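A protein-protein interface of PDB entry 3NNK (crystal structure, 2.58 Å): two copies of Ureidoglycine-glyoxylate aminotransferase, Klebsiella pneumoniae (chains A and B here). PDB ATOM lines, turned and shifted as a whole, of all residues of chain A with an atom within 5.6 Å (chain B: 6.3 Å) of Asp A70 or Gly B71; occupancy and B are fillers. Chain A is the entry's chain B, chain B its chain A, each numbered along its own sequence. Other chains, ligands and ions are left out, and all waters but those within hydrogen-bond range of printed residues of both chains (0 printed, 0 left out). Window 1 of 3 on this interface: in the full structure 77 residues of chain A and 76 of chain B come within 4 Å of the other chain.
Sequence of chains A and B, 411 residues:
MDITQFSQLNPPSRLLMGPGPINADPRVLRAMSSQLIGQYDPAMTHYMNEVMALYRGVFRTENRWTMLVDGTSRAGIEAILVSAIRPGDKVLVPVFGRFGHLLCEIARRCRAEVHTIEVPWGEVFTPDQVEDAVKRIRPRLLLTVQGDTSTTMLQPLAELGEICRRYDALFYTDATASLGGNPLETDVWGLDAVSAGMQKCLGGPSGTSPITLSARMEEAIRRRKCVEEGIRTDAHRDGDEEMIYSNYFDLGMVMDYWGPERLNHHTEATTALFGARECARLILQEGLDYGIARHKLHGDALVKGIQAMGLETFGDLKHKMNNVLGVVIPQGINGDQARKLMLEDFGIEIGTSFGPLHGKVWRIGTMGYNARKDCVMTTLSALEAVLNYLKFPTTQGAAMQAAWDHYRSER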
ATOM      1  N   LEU A  68     -21.613  -5.792   1.852  1.00  0.00           N
ATOM      2  CA  LEU A  68     -21.874  -4.417   2.274  1.00  0.00           C
ATOM      3  C   LEU A  68     -21.010  -3.388   1.552  1.00  0.00           C
ATOM      4  O   LEU A  68     -19.845  -3.644   1.238  1.00  0.00           O
ATOM      5  CB  LEU A  68     -21.663  -4.267   3.784  1.00  0.00           C
ATOM      6  CG  LEU A  68     -22.305  -5.249   4.764  1.00  0.00           C
ATOM      7  CD1 LEU A  68     -21.863  -4.908   6.181  1.00  0.00           C
ATOM      8  CD2 LEU A  68     -23.828  -5.264   4.655  1.00  0.00           C
ATOM      9  N   VAL A  69     -21.603  -2.222   1.302  1.00  0.00           N
ATOM     10  CA  VAL A  69     -20.880  -1.053   0.812  1.00  0.00           C
ATOM     11  C   VAL A  69     -20.801  -0.049   1.959  1.00  0.00           C
ATOM     12  O   VAL A  69     -21.809   0.227   2.618  1.00  0.00           O
ATOM     13  CB  VAL A  69     -21.573  -0.423  -0.426  1.00  0.00           C
ATOM     14  CG1 VAL A  69     -20.894   0.883  -0.835  1.00  0.00           C
ATOM     15  CG2 VAL A  69     -21.577  -1.401  -1.595  1.00  0.00           C
ATOM     16  N   ASP A  70     -19.605   0.477   2.208  1.00  0.00           N
ATOM     17  CA  ASP A  70     -19.401   1.432   3.296  1.00  0.00           C
ATOM     18  C   ASP A  70     -19.751   2.847   2.853  1.00  0.00           C
ATOM     19  O   ASP A  70     -18.945   3.545   2.238  1.00  0.00           O
ATOM     20  CB  ASP A  70     -17.974   1.344   3.852  1.00  0.00           C
ATOM     21  CG  ASP A  70     -17.660  -0.023   4.430  1.00  0.00           C
ATOM     22  OD1 ASP A  70     -16.630  -0.159   5.126  1.00  0.00           O
ATOM     23  OD2 ASP A  70     -18.445  -0.965   4.189  1.00  0.00           O
ATOM     24  N   GLY A  71     -20.976   3.242   3.182  1.00  0.00           N
ATOM     25  CA  GLY A  71     -21.578   4.496   2.740  1.00  0.00           C
ATOM     26  C   GLY A  71     -23.086   4.331   2.802  1.00  0.00           C
ATOM     27  O   GLY A  71     -23.581   3.212   2.948  1.00  0.00           O
ATOM     28  N   THR A  72     -23.823   5.433   2.685  1.00  0.00           N
ATOM     29  CA  THR A  72     -25.286   5.386   2.789  1.00  0.00           C
ATOM     30  C   THR A  72     -25.922   4.678   1.588  1.00  0.00           C
ATOM     31  O   THR A  72     -25.250   4.414   0.590  1.00  0.00           O
ATOM     32  CB  THR A  72     -25.906   6.793   2.993  1.00  0.00           C
ATOM     33  OG1 THR A  72     -25.774   7.566   1.793  1.00  0.00           O
ATOM     34  CG2 THR A  72     -25.220   7.520   4.142  1.00  0.00           C
ATOM     35  N   ALA A  75     -24.891   5.082  -2.024  1.00  0.00           N
ATOM     36  CA  ALA A  75     -23.512   4.714  -2.340  1.00  0.00           C
ATOM     37  C   ALA A  75     -23.464   3.303  -2.913  1.00  0.00           C
ATOM     38  O   ALA A  75     -22.669   3.015  -3.809  1.00  0.00           O
ATOM     39  CB  ALA A  75     -22.628   4.823  -1.107  1.00  0.00           C
ATOM     40  N   GLY A 207     -25.374   4.486   6.885  1.00  0.00           N
ATOM     41  CA  GLY A 207     -23.917   4.409   6.778  1.00  0.00           C
ATOM     42  C   GLY A 207     -23.412   3.130   6.135  1.00  0.00           C
ATOM     43  O   GLY A 207     -22.216   2.997   5.864  1.00  0.00           O
ATOM     44  N   THR A 208     -24.326   2.191   5.895  1.00  0.00           N
ATOM     45  CA  THR A 208     -23.999   0.906   5.283  1.00  0.00           C
ATOM     46  C   THR A 208     -25.038   0.570   4.212  1.00  0.00           C
ATOM     47  O   THR A 208     -26.225   0.867   4.374  1.00  0.00           O
ATOM     48  CB  THR A 208     -23.934  -0.217   6.344  1.00  0.00           C
ATOM     49  OG1 THR A 208     -23.034   0.167   7.392  1.00  0.00           O
ATOM     50  CG2 THR A 208     -23.451  -1.526   5.734  1.00  0.00           C
ATOM     51  N   SER A 209     -24.585  -0.035   3.115  1.00  0.00           N
ATOM     52  CA  SER A 209     -25.475  -0.422   2.025  1.00  0.00           C
ATOM     53  C   SER A 209     -25.365  -1.913   1.687  1.00  0.00           C
ATOM     54  O   SER A 209     -24.417  -2.331   1.014  1.00  0.00           O
ATOM     55  CB  SER A 209     -25.212   0.433   0.784  1.00  0.00           C
ATOM     56  OG  SER A 209     -26.199   0.200  -0.206  1.00  0.00           O
ATOM     57  N   TYR A 248     -13.057   3.459  -5.077  1.00  0.00           N
ATOM     58  CA  TYR A 248     -13.843   3.100  -3.896  1.00  0.00           C
ATOM     59  C   TYR A 248     -15.067   2.245  -4.225  1.00  0.00           C
ATOM     60  O   TYR A 248     -15.478   1.409  -3.419  1.00  0.00           O
ATOM     61  CB  TYR A 248     -14.279   4.370  -3.158  1.00  0.00           C
ATOM     62  CG  TYR A 248     -14.838   4.147  -1.769  1.00  0.00           C
ATOM     63  CD1 TYR A 248     -13.990   3.915  -0.686  1.00  0.00           C
ATOM     64  CD2 TYR A 248     -16.212   4.187  -1.534  1.00  0.00           C
ATOM     65  CE1 TYR A 248     -14.497   3.713   0.592  1.00  0.00           C
ATOM     66  CE2 TYR A 248     -16.728   3.989  -0.259  1.00  0.00           C
ATOM     67  CZ  TYR A 248     -15.864   3.753   0.799  1.00  0.00           C
ATOM     68  OH  TYR A 248     -16.359   3.560   2.065  1.00  0.00           O
ATOM     69  N   PHE A 249     -15.637   2.457  -5.410  1.00  0.00           N
ATOM     70  CA  PHE A 249     -16.879   1.786  -5.806  1.00  0.00           C
ATOM     71  C   PHE A 249     -16.707   0.651  -6.824  1.00  0.00           C
ATOM     72  O   PHE A 249     -17.699   0.114  -7.324  1.00  0.00           O
ATOM     73  CB  PHE A 249     -17.904   2.804  -6.327  1.00  0.00           C
ATOM     74  CG  PHE A 249     -18.534   3.648  -5.251  1.00  0.00           C
ATOM     75  CD1 PHE A 249     -19.014   3.071  -4.080  1.00  0.00           C
ATOM     76  CD2 PHE A 249     -18.674   5.019  -5.424  1.00  0.00           C
ATOM     77  CE1 PHE A 249     -19.604   3.851  -3.088  1.00  0.00           C
ATOM     78  CE2 PHE A 249     -19.269   5.807  -4.441  1.00  0.00           C
ATOM     79  CZ  PHE A 249     -19.731   5.222  -3.271  1.00  0.00           C
ATOM     80  N   HIS A 266      -9.971  -1.617   1.027  1.00  0.00           N
ATOM     81  CA  HIS A 266     -10.242  -0.580   2.028  1.00  0.00           C
ATOM     82  C   HIS A 266     -10.402  -1.208   3.414  1.00  0.00           C
ATOM     83  O   HIS A 266     -10.571  -2.422   3.525  1.00  0.00           O
ATOM     84  CB  HIS A 266     -11.509   0.204   1.666  1.00  0.00           C
ATOM     85  CG  HIS A 266     -12.779  -0.551   1.914  1.00  0.00           C
ATOM     86  ND1 HIS A 266     -13.439  -1.245   0.923  1.00  0.00           N
ATOM     87  CD2 HIS A 266     -13.507  -0.724   3.043  1.00  0.00           C
ATOM     88  CE1 HIS A 266     -14.519  -1.813   1.431  1.00  0.00           C
ATOM     89  NE2 HIS A 266     -14.582  -1.513   2.715  1.00  0.00           N
ATOM     90  N   THR A 267     -10.364  -0.381   4.458  1.00  0.00           N
ATOM     91  CA  THR A 267     -10.585  -0.852   5.828  1.00  0.00           C
ATOM     92  C   THR A 267     -12.079  -0.880   6.153  1.00  0.00           C
ATOM     93  O   THR A 267     -12.693   0.166   6.390  1.00  0.00           O
ATOM     94  CB  THR A 267      -9.850   0.018   6.879  1.00  0.00           C
ATOM     95  OG1 THR A 267      -8.497   0.247   6.469  1.00  0.00           O
ATOM     96  CG2 THR A 267      -9.853  -0.667   8.241  1.00  0.00           C
ATOM     97  N   GLU A 268     -12.649  -2.082   6.171  1.00  0.00           N
ATOM     98  CA  GLU A 268     -14.067  -2.278   6.466  1.00  0.00           C
ATOM     99  C   GLU A 268     -14.489  -1.574   7.756  1.00  0.00           C
ATOM    100  O   GLU A 268     -13.821  -1.695   8.787  1.00  0.00           O
ATOM    101  CB  GLU A 268     -14.396  -3.774   6.538  1.00  0.00           C
ATOM    102  CG  GLU A 268     -15.888  -4.104   6.642  1.00  0.00           C
ATOM    103  CD  GLU A 268     -16.699  -3.640   5.439  1.00  0.00           C
ATOM    104  OE1 GLU A 268     -17.868  -3.245   5.635  1.00  0.00           O
ATOM    105  OE2 GLU A 268     -16.176  -3.671   4.303  1.00  0.00           O
ATOM    106  N   ALA A 269     -15.592  -0.831   7.672  1.00  0.00           N
ATOM    107  CA  ALA A 269     -16.169  -0.137   8.819  1.00  0.00           C
ATOM    108  C   ALA A 269     -16.585  -1.137   9.898  1.00  0.00           C
ATOM    109  O   ALA A 269     -17.651  -1.753   9.814  1.00  0.00           O
ATOM    110  CB  ALA A 269     -17.356   0.716   8.375  1.00  0.00           C
ATOM    111  N   VAL B  69     -17.171  13.293   5.105  1.00  0.00           N
ATOM    112  CA  VAL B  69     -17.537  12.424   3.993  1.00  0.00           C
ATOM    113  C   VAL B  69     -17.901  11.056   4.572  1.00  0.00           C
ATOM    114  O   VAL B  69     -17.118  10.471   5.328  1.00  0.00           O
ATOM    115  CB  VAL B  69     -16.375  12.284   2.969  1.00  0.00           C
ATOM    116  CG1 VAL B  69     -16.724  11.282   1.868  1.00  0.00           C
ATOM    117  CG2 VAL B  69     -16.017  13.634   2.365  1.00  0.00           C
ATOM    118  N   ASP B  70     -19.087  10.558   4.229  1.00  0.00           N
ATOM    119  CA  ASP B  70     -19.565   9.270   4.746  1.00  0.00           C
ATOM    120  C   ASP B  70     -18.964   8.102   3.966  1.00  0.00           C
ATOM    121  O   ASP B  70     -19.502   7.672   2.941  1.00  0.00           O
ATOM    122  CB  ASP B  70     -21.098   9.202   4.738  1.00  0.00           C
ATOM    123  CG  ASP B  70     -21.742  10.300   5.569  1.00  0.00           C
ATOM    124  OD1 ASP B  70     -22.922  10.139   5.947  1.00  0.00           O
ATOM    125  OD2 ASP B  70     -21.078  11.325   5.840  1.00  0.00           O
ATOM    126  N   GLY B  71     -17.839   7.601   4.471  1.00  0.00           N
ATOM    127  CA  GLY B  71     -17.094   6.507   3.848  1.00  0.00           C
ATOM    128  C   GLY B  71     -15.705   6.422   4.454  1.00  0.00           C
ATOM    129  O   GLY B  71     -15.268   7.351   5.137  1.00  0.00           O
ATOM    130  N   THR B  72     -15.003   5.319   4.206  1.00  0.00           N
ATOM    131  CA  THR B  72     -13.654   5.131   4.749  1.00  0.00           C
ATOM    132  C   THR B  72     -12.702   6.218   4.236  1.00  0.00           C
ATOM    133  O   THR B  72     -13.018   6.922   3.276  1.00  0.00           O
ATOM    134  CB  THR B  72     -13.084   3.719   4.445  1.00  0.00           C
ATOM    135  OG1 THR B  72     -12.608   3.661   3.094  1.00  0.00           O
ATOM    136  CG2 THR B  72     -14.136   2.638   4.665  1.00  0.00           C
ATOM    137  N   SER B  73     -11.545   6.346   4.879  1.00  0.00           N
ATOM    138  CA  SER B  73     -10.576   7.408   4.572  1.00  0.00           C
ATOM    139  C   SER B  73     -10.390   7.700   3.077  1.00  0.00           C
ATOM    140  O   SER B  73     -10.328   8.864   2.672  1.00  0.00           O
ATOM    141  CB  SER B  73      -9.226   7.094   5.213  1.00  0.00           C
ATOM    142  OG  SER B  73      -9.383   6.693   6.564  1.00  0.00           O
ATOM    143  N   ARG B  74     -10.318   6.645   2.264  1.00  0.00           N
ATOM    144  CA  ARG B  74     -10.091   6.799   0.823  1.00  0.00           C
ATOM    145  C   ARG B  74     -11.317   7.269   0.033  1.00  0.00           C
ATOM    146  O   ARG B  74     -11.213   7.572  -1.159  1.00  0.00           O
ATOM    147  CB  ARG B  74      -9.479   5.531   0.213  1.00  0.00           C
ATOM    148  CG  ARG B  74     -10.397   4.319   0.153  1.00  0.00           C
ATOM    149  CD  ARG B  74      -9.598   3.070  -0.171  1.00  0.00           C
ATOM    150  NE  ARG B  74      -8.679   2.716   0.913  1.00  0.00           N
ATOM    151  CZ  ARG B  74      -7.582   1.975   0.766  1.00  0.00           C
ATOM    152  NH1 ARG B  74      -6.815   1.711   1.815  1.00  0.00           N
ATOM    153  NH2 ARG B  74      -7.243   1.499  -0.427  1.00  0.00           N
ATOM    154  N   ALA B  75     -12.471   7.321   0.697  1.00  0.00           N
ATOM    155  CA  ALA B  75     -13.682   7.877   0.096  1.00  0.00           C
ATOM    156  C   ALA B  75     -13.628   9.399   0.107  1.00  0.00           C
ATOM    157  O   ALA B  75     -14.160  10.046  -0.792  1.00  0.00           O
ATOM    158  CB  ALA B  75     -14.926   7.377   0.818  1.00  0.00           C
ATOM    159  N   GLY B  76     -12.990   9.962   1.132  1.00  0.00           N
ATOM    160  CA  GLY B  76     -12.741  11.399   1.202  1.00  0.00           C
ATOM    161  C   GLY B  76     -11.690  11.815   0.190  1.00  0.00           C
ATOM    162  O   GLY B  76     -11.772  12.900  -0.387  1.00  0.00           O
ATOM    163  N   SER B 206     -13.197   2.973  11.644  1.00  0.00           N
ATOM    164  CA  SER B 206     -13.142   3.330  10.226  1.00  0.00           C
ATOM    165  C   SER B 206     -14.546   3.463   9.643  1.00  0.00           C
ATOM    166  O   SER B 206     -15.483   2.812  10.112  1.00  0.00           O
ATOM    167  CB  SER B 206     -12.320   2.315   9.428  1.00  0.00           C
ATOM    168  OG  SER B 206     -13.004   1.080   9.301  1.00  0.00           O
ATOM    169  N   GLY B 207     -14.686   4.323   8.637  1.00  0.00           N
ATOM    170  CA  GLY B 207     -15.974   4.531   7.981  1.00  0.00           C
ATOM    171  C   GLY B 207     -16.353   5.986   7.782  1.00  0.00           C
ATOM    172  O   GLY B 207     -17.403   6.282   7.209  1.00  0.00           O
ATOM    173  N   THR B 208     -15.499   6.893   8.252  1.00  0.00           N
ATOM    174  CA  THR B 208     -15.703   8.328   8.072  1.00  0.00           C
ATOM    175  C   THR B 208     -14.387   9.001   7.681  1.00  0.00           C
ATOM    176  O   THR B 208     -13.324   8.662   8.207  1.00  0.00           O
ATOM    177  CB  THR B 208     -16.288   8.989   9.344  1.00  0.00           C
ATOM    178  OG1 THR B 208     -17.434   8.251   9.786  1.00  0.00           O
ATOM    179  CG2 THR B 208     -16.702  10.430   9.077  1.00  0.00           C
ATOM    180  N   SER B 209     -14.470   9.943   6.746  1.00  0.00           N
ATOM    181  CA  SER B 209     -13.316  10.732   6.331  1.00  0.00           C
ATOM    182  C   SER B 209     -13.586  12.228   6.511  1.00  0.00           C
ATOM    183  O   SER B 209     -14.349  12.818   5.743  1.00  0.00           O
ATOM    184  CB  SER B 209     -12.938  10.424   4.878  1.00  0.00           C
ATOM    185  OG  SER B 209     -11.893  11.273   4.430  1.00  0.00           O
ATOM    186  N   TYR B 248     -22.503  10.705  -5.427  1.00  0.00           N
ATOM    187  CA  TYR B 248     -22.147  10.583  -4.010  1.00  0.00           C
ATOM    188  C   TYR B 248     -20.922  11.422  -3.645  1.00  0.00           C
ATOM    189  O   TYR B 248     -20.889  12.053  -2.584  1.00  0.00           O
ATOM    190  CB  TYR B 248     -21.905   9.109  -3.661  1.00  0.00           C
ATOM    191  CG  TYR B 248     -21.947   8.779  -2.182  1.00  0.00           C
ATOM    192  CD1 TYR B 248     -23.151   8.797  -1.475  1.00  0.00           C
ATOM    193  CD2 TYR B 248     -20.786   8.419  -1.496  1.00  0.00           C
ATOM    194  CE1 TYR B 248     -23.195   8.487  -0.120  1.00  0.00           C
ATOM    195  CE2 TYR B 248     -20.819   8.105  -0.140  1.00  0.00           C
ATOM    196  CZ  TYR B 248     -22.027   8.141   0.542  1.00  0.00           C
ATOM    197  OH  TYR B 248     -22.072   7.830   1.884  1.00  0.00           O
ATOM    198  N   PHE B 249     -19.926  11.434  -4.528  1.00  0.00           N
ATOM    199  CA  PHE B 249     -18.676  12.156  -4.281  1.00  0.00           C
ATOM    200  C   PHE B 249     -18.640  13.576  -4.859  1.00  0.00           C
ATOM    201  O   PHE B 249     -17.579  14.207  -4.906  1.00  0.00           O
ATOM    202  CB  PHE B 249     -17.474  11.342  -4.773  1.00  0.00           C
ATOM    203  CG  PHE B 249     -17.214  10.094  -3.973  1.00  0.00           C
ATOM    204  CD1 PHE B 249     -17.219  10.123  -2.582  1.00  0.00           C
ATOM    205  CD2 PHE B 249     -16.937   8.891  -4.614  1.00  0.00           C
ATOM    206  CE1 PHE B 249     -16.973   8.972  -1.844  1.00  0.00           C
ATOM    207  CE2 PHE B 249     -16.683   7.736  -3.882  1.00  0.00           C
ATOM    208  CZ  PHE B 249     -16.703   7.776  -2.498  1.00  0.00           C
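Asp A70 touches Gly B71, and with the chains exchanged Gly A71 touches Asp B70. Gly A71 touches Tyr B248, and with the chains exchanged Tyr A248 touches Gly B71. Ala A75 touches Tyr B248, and with the chains exchanged Tyr A248 touches Ala B75. Tyr A248 touches Phe B249, and with the chains exchanged Phe A249 touches Tyr B248. Of the 20 pairs that touch across the chains among the printed residues, 13 have their exchanged pair printed and touching as well.
Of chain B, only Gly B71 (3.8 Å) and Thr B72 (3.8 Å) come within 4 Å of Asp A70. Printed residues of chain B within 4 Å of Gly A71: Asp B70 (3.8 Å) and Tyr B248 (3.5 Å). Of the printed residues of chain B, Ala A75 touches Tyr B248 (3.8 Å). Of the printed residues of chain B, Glu A268 touches Ser B206 (2.9 Å). Printed residues of chain A within 4 Å of Ser B206: Thr A267, Glu A268 and Ala A269. Thr B208 touches none of the printed residues of chain A. Of the printed residues of chain A, Phe B249 touches Tyr A248 (3.7 Å) and Phe A249 (3.3 Å). The nearest residue of chain A that does not touch Gly B71 is Gly A71 (5.0 Å). The nearest printed residue of chain A that does not touch Tyr B248 is Asp A70 (5.3 Å).
Of the 14 printed residues of chain B, 8 touch a printed residue of chain A. Of the 15 printed residues of chain A, 10 touch a printed residue of chain B. Along chain A the printed residues that touch a printed residue of chain B span positions 70 to 269.
The backbone carbonyl oxygen (O) of Gly B207 lies within hydrogen-bond range of the backbone NH (N) of Gly B71 (3.1 Å). The backbone NH (N) of Thr B208 sits close to the backbone carbonyl oxygen (O) of Gly B71 (3.2 Å). N of Ser B209 is in hydrogen-bond range of O of Gly B71. The side-chain carboxylate of Asp A70 sits at hydrogen-bond distance from the backbone NH of Ala A269. The backbone NH (N) of Gly A71 sits at hydrogen-bond distance from the backbone carbonyl oxygen (O) of Gly A207. N of Thr A208 sits at hydrogen-bond distance from O of Gly A71 (3.2 Å).
Among the printed residues, pairs that only touch across the chains: Asp A70 with Gly B71 (3.8 Å), Asp A70 with Thr B72 (3.8 Å), Gly A71 with Asp B70 (3.8 Å), Gly A71 with Tyr B248 (3.5 Å), Thr A72 with Asp B70 (3.9 Å), Ala A75 with Tyr B248 (3.8 Å), Tyr A248 with Gly B71 (3.5 Å), Tyr A248 with Arg B74 (3.7 Å), Tyr A248 with Ala B75 (3.7 Å), Tyr A248 with Phe B249 (3.7 Å), Phe A249 with Tyr B248 (3.8 Å), Phe A249 with Phe B249 (3.3 Å), His A266 with Thr B72 (3.8 Å), His A266 with Arg B74 (3.8 Å), Thr A267 with Thr B72 (3.3 Å) and Ala A269 with Ser B206 (3.3 Å).
OH of Tyr A248 sits at hydrogen-bond distance from N of Thr B72, at 3.1 Å. The side-chain hydroxyl of Ser B206 is in hydrogen-bond range of the backbone carbonyl oxygen of Thr A267 (3.1 Å). The side-chain hydroxyl of Ser B206 sits at hydrogen-bond distance from the backbone carbonyl oxygen of Glu A268, 2.9 Å away. OH of Tyr B248 sits at hydrogen-bond distance from N of Thr A72.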
